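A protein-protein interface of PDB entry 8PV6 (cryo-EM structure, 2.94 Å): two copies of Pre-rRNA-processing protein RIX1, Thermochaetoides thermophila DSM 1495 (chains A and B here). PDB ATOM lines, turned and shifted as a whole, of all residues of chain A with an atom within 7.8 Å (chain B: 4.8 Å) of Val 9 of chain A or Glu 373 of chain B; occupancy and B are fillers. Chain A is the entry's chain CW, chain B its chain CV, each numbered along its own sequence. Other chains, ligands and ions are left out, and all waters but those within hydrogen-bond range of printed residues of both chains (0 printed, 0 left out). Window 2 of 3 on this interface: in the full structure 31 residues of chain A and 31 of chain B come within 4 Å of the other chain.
O of His 32 of chain A is in hydrogen-bond range of SG of Cys 36 of chain A. The backbone carbonyl oxygen (O) of Glu 373 of chain B lies within hydrogen-bond range of the side-chain hydroxyl (OG) of Ser 376 of chain B (2.7 Å). The backbone carbonyl oxygen (O) of Leu 28 of chain A lies within hydrogen-bond range of a ring nitrogen (ND1) of His 32 of chain A (2.9 Å). The backbone carbonyl oxygen (O) of Ala 372 of chain B sits at hydrogen-bond distance from the side-chain hydroxyl (OG) of Ser 376 of chain B (3.2 Å). O of Arg 13 of chain A lies within hydrogen-bond range of OG of Ser 16 of chain A, at 3.4 Å. OE1 of Gln 307 of chain B lies close to OE2 of Glu 373 of chain B (3.1 Å).
Of the 11 printed residues of chain B, 4 touch a printed residue of chain A. Printed residues of chain B that touch a printed residue of chain A: Gln 307, Ala 372, Glu 373 and Ser 376. Hydrophobic or aromatic side chains of chain B that line the printed part of chain A: Ala 372. Along chain A the printed residues that touch a printed residue of chain B span positions 5 to 35. Among the printed residues, no Asp or Glu carboxylate lies within 4 Å of a Lys or Arg side-chain nitrogen of the other chain.
Printed residues of chain B within 4 Å of Val 9 of chain A: Glu 373. Glu 373 of chain B touches one residue of chain A. Of the printed residues of chain A, Gln 307 of chain B touches Arg 13 and Leu 28. Of the printed residues of chain B, Pro 5 of chain A touches Ala 372. Of the printed residues of chain B, Leu 28 of chain A touches Gln 307. Of the printed residues of chain B, Asp 6 of chain A touches Ser 376 (3.3 Å). Of the printed residues of chain B, His 32 of chain A touches Ser 376 (3.6 Å).
The guanidinium group (NH1) of Arg 35 of chain A is in hydrogen-bond range of the backbone carbonyl oxygen (O) of Ser 376 of chain B (2.4 Å).
O of Ala 372 of chain B touches CB of Pro 5 of chain A, 3.5 Å away. Ser 376 of chain B touches Asp 6 of chain A (CB to OD1, 3.3 Å). Arg 8 of chain A touches Ala 372 of chain B. Val 9 of chain A touches Glu 373 of chain B. Arg 13 of chain A touches Gln 307 of chain B. Leu 28 of chain A touches Gln 307 of chain B (CG to NE2, 3.4 Å). CB of Ser 376 of chain B touches NE2 of His 32 of chain A, at 3.6 Å.
No position is printed for both chains. Of the 8 pairs that touch across the chains among the printed residues, none has its exchanged pair printed and touching as well.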
ATOM      1  N   PRO A   4       1.968  18.162   0.809  1.00  0.00           N
ATOM      2  CA  PRO A   4       3.205  18.444   1.544  1.00  0.00           C
ATOM      3  C   PRO A   4       3.402  17.480   2.699  1.00  0.00           C
ATOM      4  O   PRO A   4       2.427  17.065   3.353  1.00  0.00           O
ATOM      5  CB  PRO A   4       2.995  19.879   2.046  1.00  0.00           C
ATOM      6  CG  PRO A   4       2.083  20.474   1.047  1.00  0.00           C
ATOM      7  CD  PRO A   4       1.137  19.369   0.667  1.00  0.00           C
ATOM      8  N   PRO A   5       4.653  17.080   2.956  1.00  0.00           N
ATOM      9  CA  PRO A   5       4.933  16.176   4.085  1.00  0.00           C
ATOM     10  C   PRO A   5       4.522  16.743   5.429  1.00  0.00           C
ATOM     11  O   PRO A   5       4.051  15.994   6.291  1.00  0.00           O
ATOM     12  CB  PRO A   5       6.454  15.974   4.007  1.00  0.00           C
ATOM     13  CG  PRO A   5       6.959  17.001   3.046  1.00  0.00           C
ATOM     14  CD  PRO A   5       5.843  17.318   2.125  1.00  0.00           C
ATOM     15  N   ASP A   6       4.679  18.054   5.621  1.00  0.00           N
ATOM     16  CA  ASP A   6       4.299  18.685   6.880  1.00  0.00           C
ATOM     17  C   ASP A   6       2.797  18.588   7.114  1.00  0.00           C
ATOM     18  O   ASP A   6       2.355  18.243   8.216  1.00  0.00           O
ATOM     19  CB  ASP A   6       4.754  20.141   6.874  1.00  0.00           C
ATOM     20  CG  ASP A   6       6.259  20.274   6.783  1.00  0.00           C
ATOM     21  OD1 ASP A   6       6.965  19.568   7.530  1.00  0.00           O
ATOM     22  OD2 ASP A   6       6.738  21.058   5.939  1.00  0.00           O
ATOM     23  N   LEU A   7       2.003  18.854   6.075  1.00  0.00           N
ATOM     24  CA  LEU A   7       0.552  18.751   6.192  1.00  0.00           C
ATOM     25  C   LEU A   7       0.116  17.307   6.405  1.00  0.00           C
ATOM     26  O   LEU A   7      -0.813  17.038   7.180  1.00  0.00           O
ATOM     27  CB  LEU A   7      -0.106  19.344   4.948  1.00  0.00           C
ATOM     28  CG  LEU A   7      -1.630  19.424   4.900  1.00  0.00           C
ATOM     29  CD1 LEU A   7      -2.155  20.218   6.081  1.00  0.00           C
ATOM     30  CD2 LEU A   7      -2.068  20.063   3.597  1.00  0.00           C
ATOM     31  N   ARG A   8       0.782  16.362   5.730  1.00  0.00           N
ATOM     32  CA  ARG A   8       0.460  14.949   5.920  1.00  0.00           C
ATOM     33  C   ARG A   8       0.751  14.495   7.347  1.00  0.00           C
ATOM     34  O   ARG A   8      -0.061  13.787   7.961  1.00  0.00           O
ATOM     35  CB  ARG A   8       1.246  14.101   4.922  1.00  0.00           C
ATOM     36  CG  ARG A   8       0.815  12.649   4.866  1.00  0.00           C
ATOM     37  CD  ARG A   8       1.559  11.904   3.772  1.00  0.00           C
ATOM     38  NE  ARG A   8       1.273  12.442   2.447  1.00  0.00           N
ATOM     39  CZ  ARG A   8       2.165  13.055   1.683  1.00  0.00           C
ATOM     40  NH1 ARG A   8       3.412  13.234   2.085  1.00  0.00           N
ATOM     41  NH2 ARG A   8       1.796  13.505   0.486  1.00  0.00           N
ATOM     42  N   VAL A   9       1.898  14.911   7.894  1.00  0.00           N
ATOM     43  CA  VAL A   9       2.246  14.594   9.277  1.00  0.00           C
ATOM     44  C   VAL A   9       1.244  15.220  10.237  1.00  0.00           C
ATOM     45  O   VAL A   9       0.820  14.587  11.209  1.00  0.00           O
ATOM     46  CB  VAL A   9       3.689  15.041   9.582  1.00  0.00           C
ATOM     47  CG1 VAL A   9       3.981  14.972  11.072  1.00  0.00           C
ATOM     48  CG2 VAL A   9       4.674  14.149   8.842  1.00  0.00           C
ATOM     49  N   VAL A  10       0.835  16.463   9.964  1.00  0.00           N
ATOM     50  CA  VAL A  10      -0.135  17.141  10.823  1.00  0.00           C
ATOM     51  C   VAL A  10      -1.443  16.364  10.874  1.00  0.00           C
ATOM     52  O   VAL A  10      -1.973  16.078  11.956  1.00  0.00           O
ATOM     53  CB  VAL A  10      -0.374  18.578  10.332  1.00  0.00           C
ATOM     54  CG1 VAL A  10      -1.633  19.096  10.909  1.00  0.00           C
ATOM     55  CG2 VAL A  10       0.718  19.467  10.758  1.00  0.00           C
ATOM     56  N   CYS A  11      -1.973  16.003   9.701  1.00  0.00           N
ATOM     57  CA  CYS A  11      -3.251  15.298   9.653  1.00  0.00           C
ATOM     58  C   CYS A  11      -3.155  13.928  10.313  1.00  0.00           C
ATOM     59  O   CYS A  11      -4.050  13.537  11.075  1.00  0.00           O
ATOM     60  CB  CYS A  11      -3.727  15.171   8.209  1.00  0.00           C
ATOM     61  SG  CYS A  11      -4.020  16.750   7.385  1.00  0.00           S
ATOM     62  N   HIS A  12      -2.057  13.204  10.072  1.00  0.00           N
ATOM     63  CA  HIS A  12      -1.908  11.880  10.666  1.00  0.00           C
ATOM     64  C   HIS A  12      -1.780  11.953  12.185  1.00  0.00           C
ATOM     65  O   HIS A  12      -2.411  11.167  12.904  1.00  0.00           O
ATOM     66  CB  HIS A  12      -0.700  11.166  10.063  1.00  0.00           C
ATOM     67  CG  HIS A  12      -0.220  10.009  10.880  1.00  0.00           C
ATOM     68  ND1 HIS A  12      -1.038   8.959  11.234  1.00  0.00           N
ATOM     69  CD2 HIS A  12       0.994   9.738  11.415  1.00  0.00           C
ATOM     70  CE1 HIS A  12      -0.349   8.089  11.952  1.00  0.00           C
ATOM     71  NE2 HIS A  12       0.887   8.538  12.075  1.00  0.00           N
ATOM     72  N   ARG A  13      -0.990  12.900  12.698  1.00  0.00           N
ATOM     73  CA  ARG A  13      -0.768  12.958  14.139  1.00  0.00           C
ATOM     74  C   ARG A  13      -1.989  13.511  14.861  1.00  0.00           C
ATOM     75  O   ARG A  13      -2.275  13.114  15.995  1.00  0.00           O
ATOM     76  CB  ARG A  13       0.483  13.783  14.450  1.00  0.00           C
ATOM     77  CG  ARG A  13       1.760  13.165  13.883  1.00  0.00           C
ATOM     78  CD  ARG A  13       2.172  11.854  14.536  1.00  0.00           C
ATOM     79  NE  ARG A  13       2.454  11.974  15.960  1.00  0.00           N
ATOM     80  CZ  ARG A  13       3.638  12.322  16.447  1.00  0.00           C
ATOM     81  NH1 ARG A  13       4.648  12.634  15.651  1.00  0.00           N
ATOM     82  NH2 ARG A  13       3.816  12.351  17.763  1.00  0.00           N
ATOM     83  N   LEU A  14      -2.740  14.410  14.216  1.00  0.00           N
ATOM     84  CA  LEU A  14      -3.992  14.873  14.808  1.00  0.00           C
ATOM     85  C   LEU A  14      -5.048  13.776  14.798  1.00  0.00           C
ATOM     86  O   LEU A  14      -5.893  13.710  15.699  1.00  0.00           O
ATOM     87  CB  LEU A  14      -4.501  16.115  14.077  1.00  0.00           C
ATOM     88  CG  LEU A  14      -3.862  17.453  14.461  1.00  0.00           C
ATOM     89  CD1 LEU A  14      -4.378  18.573  13.576  1.00  0.00           C
ATOM     90  CD2 LEU A  14      -4.119  17.774  15.925  1.00  0.00           C
ATOM     91  N   ALA A  15      -5.026  12.907  13.783  1.00  0.00           N
ATOM     92  CA  ALA A  15      -5.977  11.802  13.751  1.00  0.00           C
ATOM     93  C   ALA A  15      -5.626  10.731  14.779  1.00  0.00           C
ATOM     94  O   ALA A  15      -6.518  10.117  15.375  1.00  0.00           O
ATOM     95  CB  ALA A  15      -6.032  11.202  12.346  1.00  0.00           C
ATOM     96  N   SER A  16      -4.333  10.492  14.999  1.00  0.00           N
ATOM     97  CA  SER A  16      -3.903   9.387  15.849  1.00  0.00           C
ATOM     98  C   SER A  16      -3.803   9.768  17.325  1.00  0.00           C
ATOM     99  O   SER A  16      -4.098   8.945  18.198  1.00  0.00           O
ATOM    100  CB  SER A  16      -2.556   8.852  15.357  1.00  0.00           C
ATOM    101  OG  SER A  16      -1.596   9.891  15.282  1.00  0.00           O
ATOM    102  N   THR A  17      -3.385  10.994  17.619  1.00  0.00           N
ATOM    103  CA  THR A  17      -3.041  11.363  18.985  1.00  0.00           C
ATOM    104  C   THR A  17      -4.287  11.517  19.853  1.00  0.00           C
ATOM    105  O   THR A  17      -5.277  12.112  19.407  1.00  0.00           O
ATOM    106  CB  THR A  17      -2.245  12.665  19.002  1.00  0.00           C
ATOM    107  OG1 THR A  17      -1.241  12.633  17.980  1.00  0.00           O
ATOM    108  CG2 THR A  17      -1.594  12.865  20.358  1.00  0.00           C
ATOM    109  N   LEU A  28       5.367  20.259  18.359  1.00  0.00           N
ATOM    110  CA  LEU A  28       5.485  19.610  17.056  1.00  0.00           C
ATOM    111  C   LEU A  28       4.490  20.193  16.063  1.00  0.00           C
ATOM    112  O   LEU A  28       4.858  20.578  14.942  1.00  0.00           O
ATOM    113  CB  LEU A  28       5.243  18.108  17.206  1.00  0.00           C
ATOM    114  CG  LEU A  28       6.284  17.136  17.758  1.00  0.00           C
ATOM    115  CD1 LEU A  28       6.501  17.300  19.253  1.00  0.00           C
ATOM    116  CD2 LEU A  28       5.801  15.733  17.466  1.00  0.00           C
ATOM    117  N   LEU A  29       3.221  20.271  16.471  1.00  0.00           N
ATOM    118  CA  LEU A  29       2.159  20.693  15.569  1.00  0.00           C
ATOM    119  C   LEU A  29       2.313  22.152  15.173  1.00  0.00           C
ATOM    120  O   LEU A  29       2.052  22.514  14.021  1.00  0.00           O
ATOM    121  CB  LEU A  29       0.800  20.453  16.222  1.00  0.00           C
ATOM    122  CG  LEU A  29       0.478  18.995  16.547  1.00  0.00           C
ATOM    123  CD1 LEU A  29      -0.743  18.900  17.438  1.00  0.00           C
ATOM    124  CD2 LEU A  29       0.265  18.201  15.270  1.00  0.00           C
ATOM    125  N   HIS A  32       5.067  22.407  12.579  1.00  0.00           N
ATOM    126  CA  HIS A  32       4.594  21.855  11.314  1.00  0.00           C
ATOM    127  C   HIS A  32       3.617  22.797  10.609  1.00  0.00           C
ATOM    128  O   HIS A  32       3.662  22.935   9.383  1.00  0.00           O
ATOM    129  CB  HIS A  32       3.968  20.488  11.553  1.00  0.00           C
ATOM    130  CG  HIS A  32       4.956  19.367  11.609  1.00  0.00           C
ATOM    131  ND1 HIS A  32       5.298  18.738  12.785  1.00  0.00           N
ATOM    132  CD2 HIS A  32       5.671  18.759  10.634  1.00  0.00           C
ATOM    133  CE1 HIS A  32       6.187  17.793  12.534  1.00  0.00           C
ATOM    134  NE2 HIS A  32       6.430  17.785  11.236  1.00  0.00           N
ATOM    135  N   ARG A  35       5.450  25.440   9.023  1.00  0.00           N
ATOM    136  CA  ARG A  35       5.996  24.971   7.753  1.00  0.00           C
ATOM    137  C   ARG A  35       4.926  24.911   6.666  1.00  0.00           C
ATOM    138  O   ARG A  35       5.226  25.092   5.480  1.00  0.00           O
ATOM    139  CB  ARG A  35       6.666  23.614   7.936  1.00  0.00           C
ATOM    140  CG  ARG A  35       7.968  23.689   8.698  1.00  0.00           C
ATOM    141  CD  ARG A  35       8.507  22.319   9.035  1.00  0.00           C
ATOM    142  NE  ARG A  35       9.784  22.416   9.731  1.00  0.00           N
ATOM    143  CZ  ARG A  35      10.444  21.383  10.232  1.00  0.00           C
ATOM    144  NH1 ARG A  35       9.970  20.152  10.146  1.00  0.00           N
ATOM    145  NH2 ARG A  35      11.613  21.590  10.833  1.00  0.00           N
ATOM    146  N   CYS A  36       3.675  24.653   7.047  1.00  0.00           N
ATOM    147  CA  CYS A  36       2.583  24.592   6.076  1.00  0.00           C
ATOM    148  C   CYS A  36       2.165  25.981   5.605  1.00  0.00           C
ATOM    149  O   CYS A  36       1.144  26.512   6.053  1.00  0.00           O
ATOM    150  CB  CYS A  36       1.368  23.867   6.659  1.00  0.00           C
ATOM    151  SG  CYS A  36       1.629  22.132   7.053  1.00  0.00           S
ATOM    152  N   LEU A  58      -6.877  17.822   2.623  1.00  0.00           N
ATOM    153  CA  LEU A  58      -6.192  17.787   3.910  1.00  0.00           C
ATOM    154  C   LEU A  58      -6.348  19.106   4.660  1.00  0.00           C
ATOM    155  O   LEU A  58      -6.455  19.112   5.890  1.00  0.00           O
ATOM    156  CB  LEU A  58      -4.716  17.450   3.706  1.00  0.00           C
ATOM    157  CG  LEU A  58      -4.391  15.992   3.370  1.00  0.00           C
ATOM    158  CD1 LEU A  58      -2.893  15.742   3.440  1.00  0.00           C
ATOM    159  CD2 LEU A  58      -5.134  15.041   4.295  1.00  0.00           C
ATOM    160  N   LEU B 306       9.860   7.577  14.695  1.00  0.00           N
ATOM    161  CA  LEU B 306      10.842   8.342  13.931  1.00  0.00           C
ATOM    162  C   LEU B 306      11.014   9.750  14.486  1.00  0.00           C
ATOM    163  O   LEU B 306      12.137  10.263  14.553  1.00  0.00           O
ATOM    164  CB  LEU B 306      10.438   8.393  12.459  1.00  0.00           C
ATOM    165  CG  LEU B 306      11.533   8.869  11.504  1.00  0.00           C
ATOM    166  CD1 LEU B 306      12.657   7.856  11.474  1.00  0.00           C
ATOM    167  CD2 LEU B 306      10.984   9.088  10.112  1.00  0.00           C
ATOM    168  N   GLN B 307       9.916  10.388  14.892  1.00  0.00           N
ATOM    169  CA  GLN B 307      10.008  11.730  15.458  1.00  0.00           C
ATOM    170  C   GLN B 307      10.708  11.705  16.811  1.00  0.00           C
ATOM    171  O   GLN B 307      11.490  12.607  17.137  1.00  0.00           O
ATOM    172  CB  GLN B 307       8.614  12.346  15.575  1.00  0.00           C
ATOM    173  CG  GLN B 307       8.556  13.602  16.426  1.00  0.00           C
ATOM    174  CD  GLN B 307       9.102  14.831  15.716  1.00  0.00           C
ATOM    175  OE1 GLN B 307       9.461  14.783  14.540  1.00  0.00           O
ATOM    176  NE2 GLN B 307       9.181  15.940  16.441  1.00  0.00           N
ATOM    177  N   ASP B 369       4.368   7.545   4.749  1.00  0.00           N
ATOM    178  CA  ASP B 369       4.238   8.308   5.986  1.00  0.00           C
ATOM    179  C   ASP B 369       5.584   8.452   6.688  1.00  0.00           C
ATOM    180  O   ASP B 369       5.924   9.530   7.188  1.00  0.00           O
ATOM    181  CB  ASP B 369       3.213   7.641   6.903  1.00  0.00           C
ATOM    182  CG  ASP B 369       3.422   6.143   7.020  1.00  0.00           C
ATOM    183  OD1 ASP B 369       4.292   5.606   6.304  1.00  0.00           O
ATOM    184  OD2 ASP B 369       2.717   5.503   7.828  1.00  0.00           O
ATOM    185  N   GLU B 370       6.374   7.375   6.713  1.00  0.00           N
ATOM    186  CA  GLU B 370       7.693   7.443   7.331  1.00  0.00           C
ATOM    187  C   GLU B 370       8.647   8.299   6.506  1.00  0.00           C
ATOM    188  O   GLU B 370       9.466   9.040   7.068  1.00  0.00           O
ATOM    189  CB  GLU B 370       8.255   6.035   7.529  1.00  0.00           C
ATOM    190  CG  GLU B 370       9.569   5.997   8.291  1.00  0.00           C
ATOM    191  CD  GLU B 370       9.888   4.620   8.837  1.00  0.00           C
ATOM    192  OE1 GLU B 370       8.986   3.756   8.839  1.00  0.00           O
ATOM    193  OE2 GLU B 370      11.040   4.402   9.267  1.00  0.00           O
ATOM    194  N   LYS B 371       8.540   8.225   5.171  1.00  0.00           N
ATOM    195  CA  LYS B 371       9.324   9.124   4.323  1.00  0.00           C
ATOM    196  C   LYS B 371       9.008  10.586   4.607  1.00  0.00           C
ATOM    197  O   LYS B 371       9.927  11.389   4.817  1.00  0.00           O
ATOM    198  CB  LYS B 371       9.069   8.847   2.842  1.00  0.00           C
ATOM    199  CG  LYS B 371       9.533   7.507   2.326  1.00  0.00           C
ATOM    200  CD  LYS B 371       9.222   7.404   0.840  1.00  0.00           C
ATOM    201  CE  LYS B 371       9.740   6.115   0.225  1.00  0.00           C
ATOM    202  NZ  LYS B 371       9.024   4.927   0.754  1.00  0.00           N
ATOM    203  N   ALA B 372       7.724  10.938   4.642  1.00  0.00           N
ATOM    204  CA  ALA B 372       7.269  12.299   4.878  1.00  0.00           C
ATOM    205  C   ALA B 372       7.612  12.789   6.277  1.00  0.00           C
ATOM    206  O   ALA B 372       7.895  13.978   6.460  1.00  0.00           O
ATOM    207  CB  ALA B 372       5.762  12.398   4.639  1.00  0.00           C
ATOM    208  N   GLU B 373       7.589  11.898   7.269  1.00  0.00           N
ATOM    209  CA  GLU B 373       8.079  12.219   8.598  1.00  0.00           C
ATOM    210  C   GLU B 373       9.571  12.508   8.630  1.00  0.00           C
ATOM    211  O   GLU B 373       9.979  13.473   9.290  1.00  0.00           O
ATOM    212  CB  GLU B 373       7.774  11.069   9.574  1.00  0.00           C
ATOM    213  CG  GLU B 373       8.193  11.347  11.004  1.00  0.00           C
ATOM    214  CD  GLU B 373       7.327  12.399  11.662  1.00  0.00           C
ATOM    215  OE1 GLU B 373       6.142  12.510  11.289  1.00  0.00           O
ATOM    216  OE2 GLU B 373       7.834  13.132  12.534  1.00  0.00           O
ATOM    217  N   LEU B 374      10.390  11.722   7.926  1.00  0.00           N
ATOM    218  CA  LEU B 374      11.821  12.008   7.865  1.00  0.00           C
ATOM    219  C   LEU B 374      12.115  13.320   7.146  1.00  0.00           C
ATOM    220  O   LEU B 374      12.986  14.082   7.591  1.00  0.00           O
ATOM    221  CB  LEU B 374      12.563  10.859   7.181  1.00  0.00           C
ATOM    222  CG  LEU B 374      14.049  11.090   6.900  1.00  0.00           C
ATOM    223  CD1 LEU B 374      14.821  11.248   8.201  1.00  0.00           C
ATOM    224  CD2 LEU B 374      14.636   9.981   6.054  1.00  0.00           C
ATOM    225  N   TRP B 375      11.407  13.607   6.046  1.00  0.00           N
ATOM    226  CA  TRP B 375      11.660  14.847   5.318  1.00  0.00           C
ATOM    227  C   TRP B 375      11.263  16.088   6.105  1.00  0.00           C
ATOM    228  O   TRP B 375      11.748  17.180   5.793  1.00  0.00           O
ATOM    229  CB  TRP B 375      10.939  14.883   3.963  1.00  0.00           C
ATOM    230  CG  TRP B 375      11.069  13.675   3.054  1.00  0.00           C
ATOM    231  CD1 TRP B 375      10.057  13.087   2.353  1.00  0.00           C
ATOM    232  CD2 TRP B 375      12.257  12.922   2.741  1.00  0.00           C
ATOM    233  NE1 TRP B 375      10.531  12.023   1.632  1.00  0.00           N
ATOM    234  CE2 TRP B 375      11.877  11.900   1.850  1.00  0.00           C
ATOM    235  CE3 TRP B 375      13.600  13.014   3.122  1.00  0.00           C
ATOM    236  CZ2 TRP B 375      12.785  10.979   1.342  1.00  0.00           C
ATOM    237  CZ3 TRP B 375      14.497  12.097   2.618  1.00  0.00           C
ATOM    238  CH2 TRP B 375      14.087  11.094   1.736  1.00  0.00           C
ATOM    239  N   SER B 376      10.394  15.951   7.103  1.00  0.00           N
ATOM    240  CA  SER B 376      10.095  17.033   8.027  1.00  0.00           C
ATOM    241  C   SER B 376      11.022  17.066   9.230  1.00  0.00           C
ATOM    242  O   SER B 376      11.258  18.140   9.784  1.00  0.00           O
ATOM    243  CB  SER B 376       8.649  16.925   8.522  1.00  0.00           C
ATOM    244  OG  SER B 376       8.402  15.650   9.085  1.00  0.00           O
ATOM    245  N   ALA B 377      11.550  15.913   9.645  1.00  0.00           N
ATOM    246  CA  ALA B 377      12.426  15.880  10.810  1.00  0.00           C
ATOM    247  C   ALA B 377      13.837  16.350  10.473  1.00  0.00           C
ATOM    248  O   ALA B 377      14.571  16.804  11.360  1.00  0.00           O
ATOM    249  CB  ALA B 377      12.457  14.469  11.393  1.00  0.00           C
